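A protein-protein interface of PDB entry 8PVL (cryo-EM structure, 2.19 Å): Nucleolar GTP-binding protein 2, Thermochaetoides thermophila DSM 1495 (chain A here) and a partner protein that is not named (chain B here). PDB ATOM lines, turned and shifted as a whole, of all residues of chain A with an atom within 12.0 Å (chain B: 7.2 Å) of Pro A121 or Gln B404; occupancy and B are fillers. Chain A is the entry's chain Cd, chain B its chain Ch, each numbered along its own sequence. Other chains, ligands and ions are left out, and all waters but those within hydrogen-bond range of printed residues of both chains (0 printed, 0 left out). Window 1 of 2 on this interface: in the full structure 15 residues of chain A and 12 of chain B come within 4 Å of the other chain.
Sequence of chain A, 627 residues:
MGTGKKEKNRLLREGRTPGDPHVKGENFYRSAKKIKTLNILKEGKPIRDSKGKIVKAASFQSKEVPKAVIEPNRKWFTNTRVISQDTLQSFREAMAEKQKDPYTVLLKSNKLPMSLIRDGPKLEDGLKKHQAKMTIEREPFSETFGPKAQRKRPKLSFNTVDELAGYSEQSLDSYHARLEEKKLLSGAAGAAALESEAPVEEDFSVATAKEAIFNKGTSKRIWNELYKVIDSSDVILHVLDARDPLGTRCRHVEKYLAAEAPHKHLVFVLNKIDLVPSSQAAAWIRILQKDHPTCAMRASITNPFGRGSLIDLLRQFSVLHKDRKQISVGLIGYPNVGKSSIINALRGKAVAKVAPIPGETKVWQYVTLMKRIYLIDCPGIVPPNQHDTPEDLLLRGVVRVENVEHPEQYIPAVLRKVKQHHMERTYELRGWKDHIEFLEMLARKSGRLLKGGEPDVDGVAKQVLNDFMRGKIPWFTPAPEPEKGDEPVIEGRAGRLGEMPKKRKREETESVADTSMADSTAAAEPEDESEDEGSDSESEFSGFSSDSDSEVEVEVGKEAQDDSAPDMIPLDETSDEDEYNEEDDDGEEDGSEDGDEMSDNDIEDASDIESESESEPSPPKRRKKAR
Hydrophobic or aromatic side chains of chain A within 4 Å of the printed part of chain B: Pro A121, Leu A123, Leu A127 and His A130.
Of the 12 printed residues of chain B, 3 touch a printed residue of chain A.
Printed residues of chain B that touch a printed residue of chain A: Phe B382, Leu B401 and Gln B404.
Among the printed residues, no Asp or Glu carboxylate lies within 4 Å of a Lys or Arg side-chain nitrogen of the other chain.
Gln B404 touches Leu A123.
Phe B382 touches Gly A126 (CE2 to O, 3.95 Å).
Gly A126 touches Gln B404.
CD2 of Leu B401 touches CD1 of Leu A127, at 3.8 Å.
Phe B382 touches His A130 (CE2 to ND1, 3.4 Å).
Of chain B, only Gln B404 comes within 4 Å of Pro A121.
Of the printed residues of chain B, Leu A123 touches Gln B404 (3.3 Å).
Of the printed residues of chain B, Gly A126 touches Phe B382 (3.95 Å) and Gln B404 (3.8 Å).
Of the printed residues of chain B, Leu A127 touches Leu B401 (3.8 Å).
No residue of chain A comes within 4 Å of Gly B402.
No residue of chain A comes within 4 Å of His B403.
Of chain A, only Pro A121, Lys A122, Leu A123 and Gly A126 come within 4 Å of Gln B404.
No residue of chain A comes within 4 Å of Asn B405.
The backbone carbonyl oxygen of Gly A126 lies within hydrogen-bond range of a ring nitrogen (ND1) of His A130 (2.7 Å).
The side-chain amino group (NZ) of Lys A129 is in hydrogen-bond range of a ring nitrogen (NE2) of His A130.
O of Gly B402 lies close to OE1 of Gln B404 (3.5 Å).
The backbone NH (N) of Gln B404 sits at hydrogen-bond distance from the side-chain carboxylate (OD2) of Asp B425, 2.8 Å away.
The backbone carbonyl oxygen of Pro A121 lies within hydrogen-bond range of the side-chain amide nitrogen of Gln B404.
O of Lys A122 sits at hydrogen-bond distance from NE2 of Gln B404 (3.3 Å).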
ATOM      1  N   MET A  95     -40.291 -19.914  27.352  1.00  0.00           N
ATOM      2  CA  MET A  95     -39.945 -20.994  26.432  1.00  0.00           C
ATOM      3  C   MET A  95     -38.718 -21.755  26.913  1.00  0.00           C
ATOM      4  O   MET A  95     -38.640 -22.980  26.767  1.00  0.00           O
ATOM      5  CB  MET A  95     -39.701 -20.420  25.036  1.00  0.00           C
ATOM      6  CG  MET A  95     -39.798 -21.421  23.899  1.00  0.00           C
ATOM      7  SD  MET A  95     -41.415 -22.198  23.763  1.00  0.00           S
ATOM      8  CE  MET A  95     -41.035 -23.567  22.675  1.00  0.00           C
ATOM      9  N   MET A 114     -44.388 -17.589  16.955  1.00  0.00           N
ATOM     10  CA  MET A 114     -43.503 -18.600  17.523  1.00  0.00           C
ATOM     11  C   MET A 114     -42.125 -18.620  16.878  1.00  0.00           C
ATOM     12  O   MET A 114     -41.187 -19.148  17.481  1.00  0.00           O
ATOM     13  CB  MET A 114     -44.147 -19.982  17.411  1.00  0.00           C
ATOM     14  CG  MET A 114     -45.142 -20.291  18.515  1.00  0.00           C
ATOM     15  SD  MET A 114     -44.697 -19.541  20.093  1.00  0.00           S
ATOM     16  CE  MET A 114     -43.575 -20.769  20.751  1.00  0.00           C
ATOM     17  N   SER A 115     -41.975 -18.059  15.676  1.00  0.00           N
ATOM     18  CA  SER A 115     -40.654 -17.980  15.063  1.00  0.00           C
ATOM     19  C   SER A 115     -39.749 -16.996  15.795  1.00  0.00           C
ATOM     20  O   SER A 115     -38.526 -17.167  15.797  1.00  0.00           O
ATOM     21  CB  SER A 115     -40.777 -17.599  13.588  1.00  0.00           C
ATOM     22  OG  SER A 115     -41.235 -16.268  13.437  1.00  0.00           O
ATOM     23  N   LEU A 116     -40.325 -15.971  16.420  1.00  0.00           N
ATOM     24  CA  LEU A 116     -39.563 -15.002  17.197  1.00  0.00           C
ATOM     25  C   LEU A 116     -39.379 -15.415  18.651  1.00  0.00           C
ATOM     26  O   LEU A 116     -38.681 -14.719  19.393  1.00  0.00           O
ATOM     27  CB  LEU A 116     -40.242 -13.629  17.149  1.00  0.00           C
ATOM     28  CG  LEU A 116     -40.595 -13.033  15.788  1.00  0.00           C
ATOM     29  CD1 LEU A 116     -41.461 -11.799  15.969  1.00  0.00           C
ATOM     30  CD2 LEU A 116     -39.339 -12.697  15.011  1.00  0.00           C
ATOM     31  N   ILE A 117     -39.988 -16.518  19.077  1.00  0.00           N
ATOM     32  CA  ILE A 117     -39.939 -16.957  20.461  1.00  0.00           C
ATOM     33  C   ILE A 117     -39.150 -18.252  20.614  1.00  0.00           C
ATOM     34  O   ILE A 117     -38.412 -18.421  21.587  1.00  0.00           O
ATOM     35  CB  ILE A 117     -41.369 -17.103  21.031  1.00  0.00           C
ATOM     36  CG1 ILE A 117     -42.145 -15.799  20.841  1.00  0.00           C
ATOM     37  CG2 ILE A 117     -41.341 -17.475  22.503  1.00  0.00           C
ATOM     38  CD1 ILE A 117     -43.581 -15.869  21.292  1.00  0.00           C
ATOM     39  N   ARG A 118     -39.279 -19.166  19.655  1.00  0.00           N
ATOM     40  CA  ARG A 118     -38.588 -20.445  19.713  1.00  0.00           C
ATOM     41  C   ARG A 118     -37.079 -20.261  19.600  1.00  0.00           C
ATOM     42  O   ARG A 118     -36.589 -19.367  18.905  1.00  0.00           O
ATOM     43  CB  ARG A 118     -39.071 -21.363  18.593  1.00  0.00           C
ATOM     44  CG  ARG A 118     -40.106 -22.386  19.013  1.00  0.00           C
ATOM     45  CD  ARG A 118     -40.469 -23.300  17.853  1.00  0.00           C
ATOM     46  NE  ARG A 118     -41.409 -22.675  16.930  1.00  0.00           N
ATOM     47  CZ  ARG A 118     -41.069 -22.126  15.771  1.00  0.00           C
ATOM     48  NH1 ARG A 118     -39.813 -22.105  15.357  1.00  0.00           N
ATOM     49  NH2 ARG A 118     -42.015 -21.584  15.008  1.00  0.00           N
ATOM     50  N   ASP A 119     -36.347 -21.117  20.304  1.00  0.00           N
ATOM     51  CA  ASP A 119     -34.896 -21.115  20.216  1.00  0.00           C
ATOM     52  C   ASP A 119     -34.448 -21.589  18.839  1.00  0.00           C
ATOM     53  O   ASP A 119     -35.097 -22.420  18.199  1.00  0.00           O
ATOM     54  CB  ASP A 119     -34.294 -22.008  21.300  1.00  0.00           C
ATOM     55  CG  ASP A 119     -35.101 -21.988  22.583  1.00  0.00           C
ATOM     56  OD1 ASP A 119     -35.300 -20.890  23.144  1.00  0.00           O
ATOM     57  OD2 ASP A 119     -35.535 -23.069  23.031  1.00  0.00           O
ATOM     58  N   GLY A 120     -33.328 -21.041  18.380  1.00  0.00           N
ATOM     59  CA  GLY A 120     -32.807 -21.364  17.075  1.00  0.00           C
ATOM     60  C   GLY A 120     -32.217 -22.758  17.021  1.00  0.00           C
ATOM     61  O   GLY A 120     -32.011 -23.411  18.048  1.00  0.00           O
ATOM     62  N   PRO A 121     -31.944 -23.246  15.813  1.00  0.00           N
ATOM     63  CA  PRO A 121     -31.329 -24.570  15.674  1.00  0.00           C
ATOM     64  C   PRO A 121     -29.873 -24.544  16.112  1.00  0.00           C
ATOM     65  O   PRO A 121     -29.268 -23.491  16.322  1.00  0.00           O
ATOM     66  CB  PRO A 121     -31.455 -24.888  14.181  1.00  0.00           C
ATOM     67  CG  PRO A 121     -31.737 -23.594  13.509  1.00  0.00           C
ATOM     68  CD  PRO A 121     -32.217 -22.599  14.518  1.00  0.00           C
ATOM     69  N   LYS A 122     -29.316 -25.742  16.266  1.00  0.00           N
ATOM     70  CA  LYS A 122     -27.918 -25.884  16.646  1.00  0.00           C
ATOM     71  C   LYS A 122     -27.005 -25.390  15.529  1.00  0.00           C
ATOM     72  O   LYS A 122     -27.361 -25.415  14.347  1.00  0.00           O
ATOM     73  CB  LYS A 122     -27.607 -27.342  16.982  1.00  0.00           C
ATOM     74  CG  LYS A 122     -28.605 -27.974  17.939  1.00  0.00           C
ATOM     75  CD  LYS A 122     -28.348 -29.461  18.112  1.00  0.00           C
ATOM     76  CE  LYS A 122     -29.373 -30.090  19.040  1.00  0.00           C
ATOM     77  NZ  LYS A 122     -29.156 -31.555  19.197  1.00  0.00           N
ATOM     78  N   LEU A 123     -25.817 -24.921  15.922  1.00  0.00           N
ATOM     79  CA  LEU A 123     -24.898 -24.326  14.956  1.00  0.00           C
ATOM     80  C   LEU A 123     -24.349 -25.361  13.982  1.00  0.00           C
ATOM     81  O   LEU A 123     -24.108 -25.038  12.813  1.00  0.00           O
ATOM     82  CB  LEU A 123     -23.763 -23.600  15.684  1.00  0.00           C
ATOM     83  CG  LEU A 123     -22.809 -24.387  16.585  1.00  0.00           C
ATOM     84  CD1 LEU A 123     -21.476 -24.624  15.891  1.00  0.00           C
ATOM     85  CD2 LEU A 123     -22.604 -23.662  17.905  1.00  0.00           C
ATOM     86  N   GLU A 124     -24.160 -26.603  14.439  1.00  0.00           N
ATOM     87  CA  GLU A 124     -23.732 -27.669  13.538  1.00  0.00           C
ATOM     88  C   GLU A 124     -24.781 -27.936  12.467  1.00  0.00           C
ATOM     89  O   GLU A 124     -24.448 -28.078  11.284  1.00  0.00           O
ATOM     90  CB  GLU A 124     -23.435 -28.941  14.335  1.00  0.00           C
ATOM     91  CG  GLU A 124     -24.415 -29.229  15.467  1.00  0.00           C
ATOM     92  CD  GLU A 124     -23.932 -28.721  16.812  1.00  0.00           C
ATOM     93  OE1 GLU A 124     -23.022 -27.865  16.836  1.00  0.00           O
ATOM     94  OE2 GLU A 124     -24.465 -29.175  17.846  1.00  0.00           O
ATOM     95  N   ASP A 125     -26.058 -27.979  12.862  1.00  0.00           N
ATOM     96  CA  ASP A 125     -27.140 -28.161  11.899  1.00  0.00           C
ATOM     97  C   ASP A 125     -27.241 -26.975  10.949  1.00  0.00           C
ATOM     98  O   ASP A 125     -27.443 -27.160   9.744  1.00  0.00           O
ATOM     99  CB  ASP A 125     -28.464 -28.374  12.631  1.00  0.00           C
ATOM    100  CG  ASP A 125     -28.364 -29.419  13.721  1.00  0.00           C
ATOM    101  OD1 ASP A 125     -27.287 -30.037  13.859  1.00  0.00           O
ATOM    102  OD2 ASP A 125     -29.363 -29.625  14.442  1.00  0.00           O
ATOM    103  N   GLY A 126     -27.083 -25.755  11.468  1.00  0.00           N
ATOM    104  CA  GLY A 126     -27.158 -24.577  10.621  1.00  0.00           C
ATOM    105  C   GLY A 126     -26.035 -24.481   9.606  1.00  0.00           C
ATOM    106  O   GLY A 126     -26.250 -24.025   8.480  1.00  0.00           O
ATOM    107  N   LEU A 127     -24.824 -24.897   9.987  1.00  0.00           N
ATOM    108  CA  LEU A 127     -23.708 -24.889   9.048  1.00  0.00           C
ATOM    109  C   LEU A 127     -23.810 -26.031   8.040  1.00  0.00           C
ATOM    110  O   LEU A 127     -23.533 -25.838   6.846  1.00  0.00           O
ATOM    111  CB  LEU A 127     -22.387 -24.964   9.812  1.00  0.00           C
ATOM    112  CG  LEU A 127     -21.603 -23.654   9.913  1.00  0.00           C
ATOM    113  CD1 LEU A 127     -20.358 -23.843  10.759  1.00  0.00           C
ATOM    114  CD2 LEU A 127     -21.243 -23.135   8.531  1.00  0.00           C
ATOM    115  N   LYS A 128     -24.203 -27.224   8.500  1.00  0.00           N
ATOM    116  CA  LYS A 128     -24.347 -28.360   7.599  1.00  0.00           C
ATOM    117  C   LYS A 128     -25.519 -28.179   6.645  1.00  0.00           C
ATOM    118  O   LYS A 128     -25.530 -28.770   5.560  1.00  0.00           O
ATOM    119  CB  LYS A 128     -24.513 -29.645   8.408  1.00  0.00           C
ATOM    120  CG  LYS A 128     -23.957 -30.887   7.735  1.00  0.00           C
ATOM    121  CD  LYS A 128     -24.177 -32.122   8.593  1.00  0.00           C
ATOM    122  CE  LYS A 128     -25.658 -32.437   8.749  1.00  0.00           C
ATOM    123  NZ  LYS A 128     -26.417 -32.250   7.482  1.00  0.00           N
ATOM    124  N   LYS A 129     -26.511 -27.371   7.030  1.00  0.00           N
ATOM    125  CA  LYS A 129     -27.639 -27.106   6.150  1.00  0.00           C
ATOM    126  C   LYS A 129     -27.234 -26.243   4.961  1.00  0.00           C
ATOM    127  O   LYS A 129     -27.869 -26.317   3.905  1.00  0.00           O
ATOM    128  CB  LYS A 129     -28.764 -26.439   6.946  1.00  0.00           C
ATOM    129  CG  LYS A 129     -30.077 -26.278   6.193  1.00  0.00           C
ATOM    130  CD  LYS A 129     -31.134 -25.594   7.039  1.00  0.00           C
ATOM    131  CE  LYS A 129     -31.943 -24.612   6.204  1.00  0.00           C
ATOM    132  NZ  LYS A 129     -31.137 -24.024   5.095  1.00  0.00           N
ATOM    133  N   HIS A 130     -26.183 -25.436   5.100  1.00  0.00           N
ATOM    134  CA  HIS A 130     -25.761 -24.522   4.047  1.00  0.00           C
ATOM    135  C   HIS A 130     -24.435 -24.898   3.400  1.00  0.00           C
ATOM    136  O   HIS A 130     -24.004 -24.203   2.468  1.00  0.00           O
ATOM    137  CB  HIS A 130     -25.677 -23.092   4.593  1.00  0.00           C
ATOM    138  CG  HIS A 130     -26.977 -22.565   5.115  1.00  0.00           C
ATOM    139  ND1 HIS A 130     -27.388 -22.746   6.417  1.00  0.00           N
ATOM    140  CD2 HIS A 130     -27.961 -21.861   4.505  1.00  0.00           C
ATOM    141  CE1 HIS A 130     -28.568 -22.177   6.588  1.00  0.00           C
ATOM    142  NE2 HIS A 130     -28.938 -21.634   5.443  1.00  0.00           N
ATOM    143  N   GLN A 131     -23.775 -25.962   3.877  1.00  0.00           N
ATOM    144  CA  GLN A 131     -22.451 -26.323   3.365  1.00  0.00           C
ATOM    145  C   GLN A 131     -22.467 -26.673   1.877  1.00  0.00           C
ATOM    146  O   GLN A 131     -21.519 -26.349   1.154  1.00  0.00           O
ATOM    147  CB  GLN A 131     -21.884 -27.489   4.176  1.00  0.00           C
ATOM    148  CG  GLN A 131     -20.380 -27.687   4.042  1.00  0.00           C
ATOM    149  CD  GLN A 131     -19.566 -26.786   4.961  1.00  0.00           C
ATOM    150  OE1 GLN A 131     -19.812 -25.583   5.065  1.00  0.00           O
ATOM    151  NE2 GLN A 131     -18.590 -27.375   5.643  1.00  0.00           N
ATOM    152  N   ALA A 132     -23.527 -27.333   1.402  1.00  0.00           N
ATOM    153  CA  ALA A 132     -23.583 -27.752   0.000  1.00  0.00           C
ATOM    154  C   ALA A 132     -23.657 -26.555  -0.943  1.00  0.00           C
ATOM    155  O   ALA A 132     -22.892 -26.462  -1.915  1.00  0.00           O
ATOM    156  CB  ALA A 132     -24.778 -28.679  -0.217  1.00  0.00           C
ATOM    157  N   LYS A 133     -24.569 -25.621  -0.666  1.00  0.00           N
ATOM    158  CA  LYS A 133     -24.677 -24.426  -1.490  1.00  0.00           C
ATOM    159  C   LYS A 133     -23.454 -23.535  -1.337  1.00  0.00           C
ATOM    160  O   LYS A 133     -23.071 -22.858  -2.295  1.00  0.00           O
ATOM    161  CB  LYS A 133     -25.949 -23.600  -1.200  1.00  0.00           C
ATOM    162  CG  LYS A 133     -27.375 -24.231  -1.348  1.00  0.00           C
ATOM    163  CD  LYS A 133     -27.768 -25.514  -0.594  1.00  0.00           C
ATOM    164  CE  LYS A 133     -27.340 -25.508   0.868  1.00  0.00           C
ATOM    165  NZ  LYS A 133     -27.667 -26.786   1.565  1.00  0.00           N
ATOM    166  N   MET A 134     -22.815 -23.540  -0.162  1.00  0.00           N
ATOM    167  CA  MET A 134     -21.567 -22.799  -0.005  1.00  0.00           C
ATOM    168  C   MET A 134     -20.460 -23.377  -0.880  1.00  0.00           C
ATOM    169  O   MET A 134     -19.715 -22.625  -1.524  1.00  0.00           O
ATOM    170  CB  MET A 134     -21.148 -22.797   1.463  1.00  0.00           C
ATOM    171  CG  MET A 134     -19.813 -22.131   1.734  1.00  0.00           C
ATOM    172  SD  MET A 134     -19.520 -21.852   3.488  1.00  0.00           S
ATOM    173  CE  MET A 134     -21.190 -21.706   4.126  1.00  0.00           C
ATOM    174  N   GLU A 137     -21.279 -22.469  -4.513  1.00  0.00           N
ATOM    175  CA  GLU A 137     -21.001 -21.059  -4.767  1.00  0.00           C
ATOM    176  C   GLU A 137     -19.503 -20.794  -4.844  1.00  0.00           C
ATOM    177  O   GLU A 137     -19.058 -19.948  -5.627  1.00  0.00           O
ATOM    178  CB  GLU A 137     -21.639 -20.192  -3.682  1.00  0.00           C
ATOM    179  CG  GLU A 137     -23.113 -19.906  -3.900  1.00  0.00           C
ATOM    180  CD  GLU A 137     -23.795 -19.375  -2.654  1.00  0.00           C
ATOM    181  OE1 GLU A 137     -23.185 -19.438  -1.566  1.00  0.00           O
ATOM    182  OE2 GLU A 137     -24.942 -18.895  -2.762  1.00  0.00           O
ATOM    183  N   PHE B 382     -20.196 -18.026   7.549  1.00  0.00           N
ATOM    184  CA  PHE B 382     -20.951 -17.948   8.808  1.00  0.00           C
ATOM    185  C   PHE B 382     -20.003 -17.871   9.995  1.00  0.00           C
ATOM    186  O   PHE B 382     -20.460 -17.952  11.142  1.00  0.00           O
ATOM    187  CB  PHE B 382     -21.931 -19.109   9.066  1.00  0.00           C
ATOM    188  CG  PHE B 382     -23.030 -19.293   8.024  1.00  0.00           C
ATOM    189  CD1 PHE B 382     -23.090 -18.555   6.846  1.00  0.00           C
ATOM    190  CD2 PHE B 382     -24.016 -20.240   8.247  1.00  0.00           C
ATOM    191  CE1 PHE B 382     -24.099 -18.757   5.931  1.00  0.00           C
ATOM    192  CE2 PHE B 382     -25.027 -20.444   7.333  1.00  0.00           C
ATOM    193  CZ  PHE B 382     -25.069 -19.702   6.174  1.00  0.00           C
ATOM    194  N   LEU B 401     -17.564 -19.587  16.025  1.00  0.00           N
ATOM    195  CA  LEU B 401     -18.658 -20.345  15.435  1.00  0.00           C
ATOM    196  C   LEU B 401     -19.932 -20.121  16.234  1.00  0.00           C
ATOM    197  O   LEU B 401     -19.900 -20.066  17.467  1.00  0.00           O
ATOM    198  CB  LEU B 401     -18.340 -21.845  15.424  1.00  0.00           C
ATOM    199  CG  LEU B 401     -17.276 -22.394  14.481  1.00  0.00           C
ATOM    200  CD1 LEU B 401     -16.909 -23.808  14.886  1.00  0.00           C
ATOM    201  CD2 LEU B 401     -17.786 -22.378  13.063  1.00  0.00           C
ATOM    202  N   GLY B 402     -21.060 -20.042  15.536  1.00  0.00           N
ATOM    203  CA  GLY B 402     -22.334 -19.871  16.204  1.00  0.00           C
ATOM    204  C   GLY B 402     -23.336 -19.042  15.430  1.00  0.00           C
ATOM    205  O   GLY B 402     -24.542 -19.143  15.671  1.00  0.00           O
ATOM    206  N   HIS B 403     -22.859 -18.229  14.494  1.00  0.00           N
ATOM    207  CA  HIS B 403     -23.763 -17.510  13.610  1.00  0.00           C
ATOM    208  C   HIS B 403     -24.410 -18.476  12.626  1.00  0.00           C
ATOM    209  O   HIS B 403     -23.752 -19.361  12.073  1.00  0.00           O
ATOM    210  CB  HIS B 403     -23.015 -16.411  12.858  1.00  0.00           C
ATOM    211  CG  HIS B 403     -22.946 -15.112  13.598  1.00  0.00           C
ATOM    212  ND1 HIS B 403     -24.059 -14.345  13.859  1.00  0.00           N
ATOM    213  CD2 HIS B 403     -21.896 -14.446  14.132  1.00  0.00           C
ATOM    214  CE1 HIS B 403     -23.698 -13.261  14.521  1.00  0.00           C
ATOM    215  NE2 HIS B 403     -22.391 -13.298  14.699  1.00  0.00           N
ATOM    216  N   GLN B 404     -25.711 -18.307  12.414  1.00  0.00           N
ATOM    217  CA  GLN B 404     -26.468 -19.158  11.508  1.00  0.00           C
ATOM    218  C   GLN B 404     -26.571 -18.584  10.105  1.00  0.00           C
ATOM    219  O   GLN B 404     -27.263 -19.164   9.264  1.00  0.00           O
ATOM    220  CB  GLN B 404     -27.872 -19.405  12.065  1.00  0.00           C
ATOM    221  CG  GLN B 404     -27.887 -19.920  13.490  1.00  0.00           C
ATOM    222  CD  GLN B 404     -27.361 -21.334  13.599  1.00  0.00           C
ATOM    223  OE1 GLN B 404     -26.163 -21.551  13.755  1.00  0.00           O
ATOM    224  NE2 GLN B 404     -28.258 -22.305  13.511  1.00  0.00           N
ATOM    225  N   ASN B 405     -25.909 -17.466   9.840  1.00  0.00           N
ATOM    226  CA  ASN B 405     -25.918 -16.839   8.527  1.00  0.00           C
ATOM    227  C   ASN B 405     -24.621 -16.048   8.397  1.00  0.00           C
ATOM    228  O   ASN B 405     -23.726 -16.160   9.241  1.00  0.00           O
ATOM    229  CB  ASN B 405     -27.169 -15.974   8.346  1.00  0.00           C
ATOM    230  CG  ASN B 405     -27.574 -15.828   6.895  1.00  0.00           C
ATOM    231  OD1 ASN B 405     -26.752 -15.973   5.993  1.00  0.00           O
ATOM    232  ND2 ASN B 405     -28.850 -15.553   6.661  1.00  0.00           N
ATOM    233  N   LYS B 406     -24.513 -15.264   7.326  1.00  0.00           N
ATOM    234  CA  LYS B 406     -23.295 -14.518   7.043  1.00  0.00           C
ATOM    235  C   LYS B 406     -23.024 -13.485   8.129  1.00  0.00           C
ATOM    236  O   LYS B 406     -23.935 -12.801   8.600  1.00  0.00           O
ATOM    237  CB  LYS B 406     -23.413 -13.820   5.688  1.00  0.00           C
ATOM    238  CG  LYS B 406     -23.829 -14.729   4.550  1.00  0.00           C
ATOM    239  CD  LYS B 406     -24.002 -13.954   3.255  1.00  0.00           C
ATOM    240  CE  LYS B 406     -25.227 -13.063   3.301  1.00  0.00           C
ATOM    241  NZ  LYS B 406     -26.487 -13.854   3.332  1.00  0.00           N
ATOM    242  N   VAL B 407     -21.767 -13.387   8.541  1.00  0.00           N
ATOM    243  CA  VAL B 407     -21.350 -12.365   9.492  1.00  0.00           C
ATOM    244  C   VAL B 407     -20.992 -11.117   8.700  1.00  0.00           C
ATOM    245  O   VAL B 407     -20.082 -11.141   7.866  1.00  0.00           O
ATOM    246  CB  VAL B 407     -20.167 -12.838  10.350  1.00  0.00           C
ATOM    247  CG1 VAL B 407     -20.034 -11.957  11.582  1.00  0.00           C
ATOM    248  CG2 VAL B 407     -20.343 -14.292  10.744  1.00  0.00           C
ATOM    249  N   TRP B 424     -26.162 -11.836   9.624  1.00  0.00           N
ATOM    250  CA  TRP B 424     -27.369 -11.793   8.809  1.00  0.00           C
ATOM    251  C   TRP B 424     -28.492 -12.661   9.361  1.00  0.00           C
ATOM    252  O   TRP B 424     -29.574 -12.693   8.768  1.00  0.00           O
ATOM    253  CB  TRP B 424     -27.056 -12.213   7.372  1.00  0.00           C
ATOM    254  CG  TRP B 424     -26.348 -11.164   6.573  1.00  0.00           C
ATOM    255  CD1 TRP B 424     -25.166 -10.557   6.878  1.00  0.00           C
ATOM    256  CD2 TRP B 424     -26.779 -10.597   5.331  1.00  0.00           C
ATOM    257  NE1 TRP B 424     -24.833  -9.651   5.906  1.00  0.00           N
ATOM    258  CE2 TRP B 424     -25.807  -9.654   4.944  1.00  0.00           C
ATOM    259  CE3 TRP B 424     -27.891 -10.795   4.509  1.00  0.00           C
ATOM    260  CZ2 TRP B 424     -25.914  -8.912   3.773  1.00  0.00           C
ATOM    261  CZ3 TRP B 424     -27.995 -10.056   3.346  1.00  0.00           C
ATOM    262  CH2 TRP B 424     -27.012  -9.127   2.988  1.00  0.00           C
ATOM    263  N   ASP B 425     -28.265 -13.363  10.474  1.00  0.00           N
ATOM    264  CA  ASP B 425     -29.304 -14.134  11.145  1.00  0.00           C
ATOM    265  C   ASP B 425     -30.039 -13.320  12.201  1.00  0.00           C
ATOM    266  O   ASP B 425     -30.532 -13.889  13.185  1.00  0.00           O
ATOM    267  CB  ASP B 425     -28.706 -15.399  11.760  1.00  0.00           C
ATOM    268  CG  ASP B 425     -27.490 -15.113  12.618  1.00  0.00           C
ATOM    269  OD1 ASP B 425     -26.988 -13.972  12.585  1.00  0.00           O
ATOM    270  OD2 ASP B 425     -27.036 -16.033  13.328  1.00  0.00           O
ATOM    271  N   SER B 427     -28.874 -11.361  14.427  1.00  0.00           N
ATOM    272  CA  SER B 427     -28.265 -11.531  15.735  1.00  0.00           C
ATOM    273  C   SER B 427     -26.921 -10.820  15.828  1.00  0.00           C
ATOM    274  O   SER B 427     -26.143 -10.760  14.866  1.00  0.00           O
ATOM    275  CB  SER B 427     -28.083 -13.015  16.082  1.00  0.00           C
ATOM    276  OG  SER B 427     -26.989 -13.573  15.380  1.00  0.00           O
ATOM    277  N   LYS B 429     -23.578 -11.138  18.376  1.00  0.00           N
ATOM    278  CA  LYS B 429     -22.966 -12.089  19.289  1.00  0.00           C
ATOM    279  C   LYS B 429     -21.736 -11.485  19.950  1.00  0.00           C
ATOM    280  O   LYS B 429     -21.071 -10.606  19.390  1.00  0.00           O
ATOM    281  CB  LYS B 429     -22.593 -13.386  18.570  1.00  0.00           C
ATOM    282  CG  LYS B 429     -23.786 -14.275  18.305  1.00  0.00           C
ATOM    283  CD  LYS B 429     -23.388 -15.579  17.655  1.00  0.00           C
ATOM    284  CE  LYS B 429     -24.546 -16.551  17.687  1.00  0.00           C
ATOM    285  NZ  LYS B 429     -25.715 -16.028  16.938  1.00  0.00           N
